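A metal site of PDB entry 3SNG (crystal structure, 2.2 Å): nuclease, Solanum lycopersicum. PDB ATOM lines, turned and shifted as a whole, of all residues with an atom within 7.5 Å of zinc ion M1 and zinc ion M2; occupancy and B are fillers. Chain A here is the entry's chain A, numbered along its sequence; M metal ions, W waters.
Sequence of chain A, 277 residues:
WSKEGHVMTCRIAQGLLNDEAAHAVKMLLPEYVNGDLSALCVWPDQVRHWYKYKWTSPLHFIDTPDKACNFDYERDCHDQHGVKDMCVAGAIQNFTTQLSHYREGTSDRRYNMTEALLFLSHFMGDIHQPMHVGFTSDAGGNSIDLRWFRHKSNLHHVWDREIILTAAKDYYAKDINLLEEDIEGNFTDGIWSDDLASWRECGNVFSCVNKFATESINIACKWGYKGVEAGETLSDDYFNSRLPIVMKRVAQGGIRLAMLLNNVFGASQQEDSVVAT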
ATOM      1  N   TRP A   1      13.278   9.517  -0.529  1.00  0.00           N
ATOM      2  CA  TRP A   1      13.160   8.255  -1.258  1.00  0.00           C
ATOM      3  C   TRP A   1      13.711   8.390  -2.674  1.00  0.00           C
ATOM      4  O   TRP A   1      13.797   9.504  -3.226  1.00  0.00           O
ATOM      5  CB  TRP A   1      11.698   7.845  -1.407  1.00  0.00           C
ATOM      6  CG  TRP A   1      10.903   7.763  -0.176  1.00  0.00           C
ATOM      7  CD1 TRP A   1       9.971   8.622   0.218  1.00  0.00           C
ATOM      8  CD2 TRP A   1      10.906   6.696   0.799  1.00  0.00           C
ATOM      9  NE1 TRP A   1       9.402   8.214   1.384  1.00  0.00           N
ATOM     10  CE2 TRP A   1       9.960   7.022   1.770  1.00  0.00           C
ATOM     11  CE3 TRP A   1      11.629   5.513   0.945  1.00  0.00           C
ATOM     12  CZ2 TRP A   1       9.697   6.223   2.880  1.00  0.00           C
ATOM     13  CZ3 TRP A   1      11.375   4.701   2.048  1.00  0.00           C
ATOM     14  CH2 TRP A   1      10.421   5.068   3.002  1.00  0.00           C
ATOM     15  N   SER A   2      14.046   7.255  -3.250  1.00  0.00           N
ATOM     16  CA  SER A   2      14.232   7.162  -4.710  1.00  0.00           C
ATOM     17  C   SER A   2      12.849   7.024  -5.343  1.00  0.00           C
ATOM     18  O   SER A   2      11.813   7.180  -4.675  1.00  0.00           O
ATOM     19  CB  SER A   2      15.106   5.970  -5.065  1.00  0.00           C
ATOM     20  OG  SER A   2      16.349   6.065  -4.410  1.00  0.00           O
ATOM     21  N   LYS A   3      12.828   6.740  -6.634  1.00  0.00           N
ATOM     22  CA  LYS A   3      11.618   6.842  -7.432  1.00  0.00           C
ATOM     23  C   LYS A   3      10.448   6.054  -6.872  1.00  0.00           C
ATOM     24  O   LYS A   3       9.334   6.601  -6.734  1.00  0.00           O
ATOM     25  CB  LYS A   3      11.948   6.435  -8.886  1.00  0.00           C
ATOM     26  CG  LYS A   3      10.754   6.138  -9.762  1.00  0.00           C
ATOM     27  CD  LYS A   3      11.173   5.577 -11.141  1.00  0.00           C
ATOM     28  CE  LYS A   3      11.475   4.070 -11.082  1.00  0.00           C
ATOM     29  NZ  LYS A   3      11.541   3.447 -12.441  1.00  0.00           N
ATOM     30  N   GLY A   5       9.575   4.950  -3.797  1.00  0.00           N
ATOM     31  CA  GLY A   5       8.900   5.467  -2.582  1.00  0.00           C
ATOM     32  C   GLY A   5       8.021   6.680  -2.867  1.00  0.00           C
ATOM     33  O   GLY A   5       6.951   6.823  -2.310  1.00  0.00           O
ATOM     34  N   HIS A   6       8.514   7.578  -3.722  1.00  0.00           N
ATOM     35  CA  HIS A   6       7.748   8.769  -4.120  1.00  0.00           C
ATOM     36  C   HIS A   6       6.511   8.416  -4.916  1.00  0.00           C
ATOM     37  O   HIS A   6       5.408   8.959  -4.671  1.00  0.00           O
ATOM     38  CB  HIS A   6       8.669   9.722  -4.891  1.00  0.00           C
ATOM     39  CG  HIS A   6       9.632  10.434  -3.985  1.00  0.00           C
ATOM     40  ND1 HIS A   6       9.210  11.273  -2.986  1.00  0.00           N
ATOM     41  CD2 HIS A   6      10.982  10.420  -3.923  1.00  0.00           C
ATOM     42  CE1 HIS A   6      10.257  11.743  -2.338  1.00  0.00           C
ATOM     43  NE2 HIS A   6      11.347  11.221  -2.861  1.00  0.00           N
ATOM     44  N   CYS A  41       6.170  13.026  -9.300  1.00  0.00           N
ATOM     45  CA  CYS A  41       6.601  13.217  -7.911  1.00  0.00           C
ATOM     46  C   CYS A  41       8.111  13.076  -7.750  1.00  0.00           C
ATOM     47  O   CYS A  41       8.676  13.498  -6.731  1.00  0.00           O
ATOM     48  CB  CYS A  41       5.843  12.277  -6.964  1.00  0.00           C
ATOM     49  SG  CYS A  41       6.161  10.590  -7.336  1.00  0.00           S
ATOM     50  N   VAL A  42       8.758  12.530  -8.770  1.00  0.00           N
ATOM     51  CA  VAL A  42      10.187  12.451  -8.804  1.00  0.00           C
ATOM     52  C   VAL A  42      10.805  13.741  -9.303  1.00  0.00           C
ATOM     53  O   VAL A  42      11.993  13.951  -9.126  1.00  0.00           O
ATOM     54  CB  VAL A  42      10.673  11.261  -9.687  1.00  0.00           C
ATOM     55  CG1 VAL A  42      12.168  11.135  -9.646  1.00  0.00           C
ATOM     56  CG2 VAL A  42      10.088   9.978  -9.150  1.00  0.00           C
ATOM     57  N   PRO A  44      11.237  16.785  -8.405  1.00  0.00           N
ATOM     58  CA  PRO A  44      12.235  17.530  -7.639  1.00  0.00           C
ATOM     59  C   PRO A  44      13.637  16.883  -7.554  1.00  0.00           C
ATOM     60  O   PRO A  44      14.633  17.587  -7.439  1.00  0.00           O
ATOM     61  CB  PRO A  44      11.593  17.644  -6.269  1.00  0.00           C
ATOM     62  CG  PRO A  44      10.141  17.671  -6.557  1.00  0.00           C
ATOM     63  CD  PRO A  44       9.982  16.652  -7.662  1.00  0.00           C
ATOM     64  N   ASP A  45      13.738  15.561  -7.603  1.00  0.00           N
ATOM     65  CA  ASP A  45      15.021  14.895  -7.671  1.00  0.00           C
ATOM     66  C   ASP A  45      15.772  15.089  -9.011  1.00  0.00           C
ATOM     67  O   ASP A  45      16.999  14.934  -9.088  1.00  0.00           O
ATOM     68  CB  ASP A  45      14.872  13.399  -7.314  1.00  0.00           C
ATOM     69  CG  ASP A  45      14.827  13.164  -5.774  1.00  0.00           C
ATOM     70  OD1 ASP A  45      15.152  14.132  -5.026  1.00  0.00           O
ATOM     71  OD2 ASP A  45      14.484  12.052  -5.321  1.00  0.00           O
ATOM     72  N   ARG A  48      16.808  19.192  -8.856  1.00  0.00           N
ATOM     73  CA  ARG A  48      17.749  19.651  -7.838  1.00  0.00           C
ATOM     74  C   ARG A  48      19.185  19.827  -8.373  1.00  0.00           C
ATOM     75  O   ARG A  48      19.991  20.553  -7.801  1.00  0.00           O
ATOM     76  CB  ARG A  48      17.796  18.706  -6.649  1.00  0.00           C
ATOM     77  CG  ARG A  48      18.416  17.375  -6.937  1.00  0.00           C
ATOM     78  CD  ARG A  48      18.174  16.366  -5.846  1.00  0.00           C
ATOM     79  NE  ARG A  48      18.877  16.665  -4.609  1.00  0.00           N
ATOM     80  CZ  ARG A  48      18.771  15.938  -3.489  1.00  0.00           C
ATOM     81  NH1 ARG A  48      18.006  14.853  -3.461  1.00  0.00           N
ATOM     82  NH2 ARG A  48      19.456  16.270  -2.396  1.00  0.00           N
ATOM     83  N   THR A  56      17.123  24.427  -4.152  1.00  0.00           N
ATOM     84  CA  THR A  56      16.295  23.300  -3.667  1.00  0.00           C
ATOM     85  C   THR A  56      17.042  22.152  -3.029  1.00  0.00           C
ATOM     86  O   THR A  56      16.418  21.283  -2.400  1.00  0.00           O
ATOM     87  CB  THR A  56      15.414  22.678  -4.772  1.00  0.00           C
ATOM     88  OG1 THR A  56      16.224  21.922  -5.712  1.00  0.00           O
ATOM     89  CG2 THR A  56      14.623  23.757  -5.485  1.00  0.00           C
ATOM     90  N   SER A  57      18.351  22.094  -3.222  1.00  0.00           N
ATOM     91  CA  SER A  57      19.119  20.947  -2.767  1.00  0.00           C
ATOM     92  C   SER A  57      19.016  20.713  -1.242  1.00  0.00           C
ATOM     93  O   SER A  57      18.715  19.610  -0.821  1.00  0.00           O
ATOM     94  CB  SER A  57      20.572  21.090  -3.158  1.00  0.00           C
ATOM     95  OG  SER A  57      21.336  20.149  -2.450  1.00  0.00           O
ATOM     96  N   LEU A  59      16.638  21.337   0.578  1.00  0.00           N
ATOM     97  CA  LEU A  59      15.265  21.149   0.995  1.00  0.00           C
ATOM     98  C   LEU A  59      14.808  19.679   1.039  1.00  0.00           C
ATOM     99  O   LEU A  59      13.659  19.405   1.432  1.00  0.00           O
ATOM    100  CB  LEU A  59      14.333  21.893   0.092  1.00  0.00           C
ATOM    101  CG  LEU A  59      14.581  23.357  -0.037  1.00  0.00           C
ATOM    102  CD1 LEU A  59      13.485  24.007  -0.866  1.00  0.00           C
ATOM    103  CD2 LEU A  59      14.708  23.990   1.392  1.00  0.00           C
ATOM    104  N   HIS A  60      15.652  18.742   0.611  1.00  0.00           N
ATOM    105  CA  HIS A  60      15.244  17.320   0.620  1.00  0.00           C
ATOM    106  C   HIS A  60      15.456  16.579   1.950  1.00  0.00           C
ATOM    107  O   HIS A  60      14.986  15.417   2.116  1.00  0.00           O
ATOM    108  CB  HIS A  60      15.982  16.555  -0.483  1.00  0.00           C
ATOM    109  CG  HIS A  60      15.575  16.943  -1.859  1.00  0.00           C
ATOM    110  ND1 HIS A  60      14.810  16.128  -2.669  1.00  0.00           N
ATOM    111  CD2 HIS A  60      15.777  18.085  -2.541  1.00  0.00           C
ATOM    112  CE1 HIS A  60      14.588  16.754  -3.810  1.00  0.00           C
ATOM    113  NE2 HIS A  60      15.161  17.954  -3.757  1.00  0.00           N
ATOM    114  N   PHE A  61      16.148  17.204   2.902  1.00  0.00           N
ATOM    115  CA  PHE A  61      16.593  16.487   4.091  1.00  0.00           C
ATOM    116  C   PHE A  61      16.742  17.414   5.289  1.00  0.00           C
ATOM    117  O   PHE A  61      16.509  18.597   5.197  1.00  0.00           O
ATOM    118  CB  PHE A  61      17.924  15.765   3.824  1.00  0.00           C
ATOM    119  CG  PHE A  61      19.046  16.686   3.401  1.00  0.00           C
ATOM    120  CD1 PHE A  61      19.783  17.374   4.346  1.00  0.00           C
ATOM    121  CD2 PHE A  61      19.364  16.844   2.078  1.00  0.00           C
ATOM    122  CE1 PHE A  61      20.768  18.255   3.976  1.00  0.00           C
ATOM    123  CE2 PHE A  61      20.382  17.717   1.696  1.00  0.00           C
ATOM    124  CZ  PHE A  61      21.095  18.411   2.655  1.00  0.00           C
ATOM    125  N   VAL A  88      13.822  20.172   4.749  1.00  0.00           N
ATOM    126  CA  VAL A  88      12.573  19.559   4.244  1.00  0.00           C
ATOM    127  C   VAL A  88      11.366  19.997   5.091  1.00  0.00           C
ATOM    128  O   VAL A  88      10.283  20.257   4.535  1.00  0.00           O
ATOM    129  CB  VAL A  88      12.703  18.038   4.082  1.00  0.00           C
ATOM    130  CG1 VAL A  88      12.755  17.351   5.447  1.00  0.00           C
ATOM    131  CG2 VAL A  88      11.544  17.469   3.210  1.00  0.00           C
ATOM    132  N   HIS A 122       6.587  15.690  -3.147  1.00  0.00           N
ATOM    133  CA  HIS A 122       7.868  15.041  -3.010  1.00  0.00           C
ATOM    134  C   HIS A 122       8.416  15.181  -1.583  1.00  0.00           C
ATOM    135  O   HIS A 122       8.868  14.211  -0.984  1.00  0.00           O
ATOM    136  CB  HIS A 122       8.847  15.658  -4.003  1.00  0.00           C
ATOM    137  CG  HIS A 122      10.200  15.014  -4.003  1.00  0.00           C
ATOM    138  ND1 HIS A 122      10.536  14.008  -4.877  1.00  0.00           N
ATOM    139  CD2 HIS A 122      11.297  15.238  -3.237  1.00  0.00           C
ATOM    140  CE1 HIS A 122      11.781  13.619  -4.637  1.00  0.00           C
ATOM    141  NE2 HIS A 122      12.266  14.341  -3.637  1.00  0.00           N
ATOM    142  N   PHE A 123       8.411  16.391  -1.046  1.00  0.00           N
ATOM    143  CA  PHE A 123       9.026  16.622   0.271  1.00  0.00           C
ATOM    144  C   PHE A 123       8.261  15.923   1.393  1.00  0.00           C
ATOM    145  O   PHE A 123       8.872  15.481   2.350  1.00  0.00           O
ATOM    146  CB  PHE A 123       9.197  18.114   0.545  1.00  0.00           C
ATOM    147  CG  PHE A 123      10.215  18.780  -0.371  1.00  0.00           C
ATOM    148  CD1 PHE A 123      11.366  18.125  -0.746  1.00  0.00           C
ATOM    149  CD2 PHE A 123      10.004  20.039  -0.863  1.00  0.00           C
ATOM    150  CE1 PHE A 123      12.314  18.718  -1.608  1.00  0.00           C
ATOM    151  CE2 PHE A 123      10.969  20.658  -1.735  1.00  0.00           C
ATOM    152  CZ  PHE A 123      12.084  19.980  -2.106  1.00  0.00           C
ATOM    153  N   GLY A 125       7.094  13.052   1.114  1.00  0.00           N
ATOM    154  CA  GLY A 125       7.755  11.761   1.039  1.00  0.00           C
ATOM    155  C   GLY A 125       9.108  11.817   1.728  1.00  0.00           C
ATOM    156  O   GLY A 125       9.387  11.014   2.594  1.00  0.00           O
ATOM    157  N   ASP A 126       9.937  12.790   1.367  1.00  0.00           N
ATOM    158  CA  ASP A 126      11.267  12.860   1.923  1.00  0.00           C
ATOM    159  C   ASP A 126      11.278  12.952   3.466  1.00  0.00           C
ATOM    160  O   ASP A 126      12.091  12.291   4.098  1.00  0.00           O
ATOM    161  CB  ASP A 126      12.101  14.004   1.281  1.00  0.00           C
ATOM    162  CG  ASP A 126      12.711  13.601  -0.080  1.00  0.00           C
ATOM    163  OD1 ASP A 126      12.654  12.430  -0.409  1.00  0.00           O
ATOM    164  OD2 ASP A 126      13.335  14.424  -0.776  1.00  0.00           O
ATOM    165  N   ILE A 127      10.397  13.756   4.058  1.00  0.00           N
ATOM    166  CA  ILE A 127      10.454  13.942   5.496  1.00  0.00           C
ATOM    167  C   ILE A 127      10.125  12.635   6.229  1.00  0.00           C
ATOM    168  O   ILE A 127      10.539  12.459   7.339  1.00  0.00           O
ATOM    169  CB  ILE A 127       9.529  15.053   5.984  1.00  0.00           C
ATOM    170  CG1 ILE A 127       9.954  15.503   7.400  1.00  0.00           C
ATOM    171  CG2 ILE A 127       8.076  14.630   5.943  1.00  0.00           C
ATOM    172  CD1 ILE A 127       9.321  16.828   7.841  1.00  0.00           C
ATOM    173  N   GLN A 129      11.099   9.607   5.027  1.00  0.00           N
ATOM    174  CA  GLN A 129      12.210   8.658   4.838  1.00  0.00           C
ATOM    175  C   GLN A 129      13.182   8.867   6.000  1.00  0.00           C
ATOM    176  O   GLN A 129      13.832   9.913   6.094  1.00  0.00           O
ATOM    177  CB  GLN A 129      12.927   8.910   3.501  1.00  0.00           C
ATOM    178  CG  GLN A 129      13.597   7.642   2.853  1.00  0.00           C
ATOM    179  CD  GLN A 129      14.879   7.181   3.550  1.00  0.00           C
ATOM    180  OE1 GLN A 129      14.859   6.925   4.766  1.00  0.00           O
ATOM    181  NE2 GLN A 129      15.993   7.096   2.799  1.00  0.00           N
ATOM    182  N   HIS A 132      16.528  10.550   5.597  1.00  0.00           N
ATOM    183  CA  HIS A 132      16.487  11.980   5.241  1.00  0.00           C
ATOM    184  C   HIS A 132      16.497  12.925   6.453  1.00  0.00           C
ATOM    185  O   HIS A 132      16.601  14.148   6.277  1.00  0.00           O
ATOM    186  CB  HIS A 132      15.275  12.279   4.345  1.00  0.00           C
ATOM    187  CG  HIS A 132      15.513  11.922   2.912  1.00  0.00           C
ATOM    188  ND1 HIS A 132      15.496  12.857   1.909  1.00  0.00           N
ATOM    189  CD2 HIS A 132      15.882  10.761   2.349  1.00  0.00           C
ATOM    190  CE1 HIS A 132      15.804  12.263   0.755  1.00  0.00           C
ATOM    191  NE2 HIS A 132      16.031  11.001   1.002  1.00  0.00           N
ATOM    192  N   HIS A 156      22.094   5.137   3.385  1.00  0.00           N
ATOM    193  CA  HIS A 156      21.002   6.004   2.861  1.00  0.00           C
ATOM    194  C   HIS A 156      20.207   5.325   1.754  1.00  0.00           C
ATOM    195  O   HIS A 156      18.951   5.287   1.776  1.00  0.00           O
ATOM    196  CB  HIS A 156      21.565   7.306   2.377  1.00  0.00           C
ATOM    197  CG  HIS A 156      20.518   8.345   2.062  1.00  0.00           C
ATOM    198  ND1 HIS A 156      20.152   9.327   2.951  1.00  0.00           N
ATOM    199  CD2 HIS A 156      19.788   8.561   0.937  1.00  0.00           C
ATOM    200  CE1 HIS A 156      19.245  10.115   2.393  1.00  0.00           C
ATOM    201  NE2 HIS A 156      18.995   9.667   1.178  1.00  0.00           N
ATOM    202  N   ASP A 160      16.387   4.546   0.925  1.00  0.00           N
ATOM    203  CA  ASP A 160      15.780   5.237  -0.230  1.00  0.00           C
ATOM    204  C   ASP A 160      15.211   4.255  -1.238  1.00  0.00           C
ATOM    205  O   ASP A 160      14.195   4.547  -1.864  1.00  0.00           O
ATOM    206  CB  ASP A 160      16.794   6.081  -0.984  1.00  0.00           C
ATOM    207  CG  ASP A 160      16.825   7.550  -0.566  1.00  0.00           C
ATOM    208  OD1 ASP A 160      16.059   8.034   0.276  1.00  0.00           O
ATOM    209  OD2 ASP A 160      17.640   8.244  -1.122  1.00  0.00           O
HETATM  210 ZN    ZN M   1      13.163  11.120  -1.969  1.00  0.00          ZN
HETATM  211 ZN    ZN M   2      14.024  14.242  -2.615  1.00  0.00          ZN
HETATM  212 ZN    ZN M   3      17.548  10.163  -0.253  1.00  0.00          ZN
HETATM  213  O   HOH W   1      14.428  12.350  -2.520  1.00  0.00           O
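Zinc ion M1 is bound by water W1, a ring nitrogen (NE2) of His 6, the side-chain carboxylate of Asp 126, the backbone carbonyl oxygen of Trp 1 and the backbone nitrogen of Trp 1.
CE1 of His 132 touches zinc ion M1 (3.96 Å).
The nearest printed residue that does not touch zinc ion M1 is Ser 2 (4.2 Å).
Zinc ion M2 is bound by water W1 (1.9 Å), OD2 of Asp 126 (2.0 Å), NE2 of His 122 (2.0 Å) and ND1 of His 60 (2.0 Å).
Zinc ion M2 has four donor atoms within binding distance.
Slightly farther from zinc ion M2 lies the side-chain carboxylate (OD1) of Asp 45 (2.7 Å).
O of His 6 sits at hydrogen-bond distance from SG of Cys 41.
A ring nitrogen (NE2) of His 122 sits close to the side-chain carboxylate (OD1) of Asp 45 (3.2 Å).
ND1 of His 122 is in hydrogen-bond range of O of Cys 41, 2.7 Å away.
A ring nitrogen (ND1) of His 60 sits close to the side-chain carboxylate (OD1) of Asp 45, 3.1 Å away.
O of His 60 sits at hydrogen-bond distance from ND1 of His 132.
The backbone NH (N) of Trp 1 sits close to the side-chain carboxylate (OD1) of Asp 160 (3.3 Å).
The indole nitrogen (NE1) of Trp 1 sits at hydrogen-bond distance from the backbone carbonyl oxygen (O) of Gly 125 (3.1 Å).
The side-chain carboxylate of Asp 45 lies within salt-bridge range of the guanidinium group of Arg 48 (3.3 Å).
Four residues have an atom within 4 Å of zinc ion M2: Asp 45, His 60, His 122 and Asp 126.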
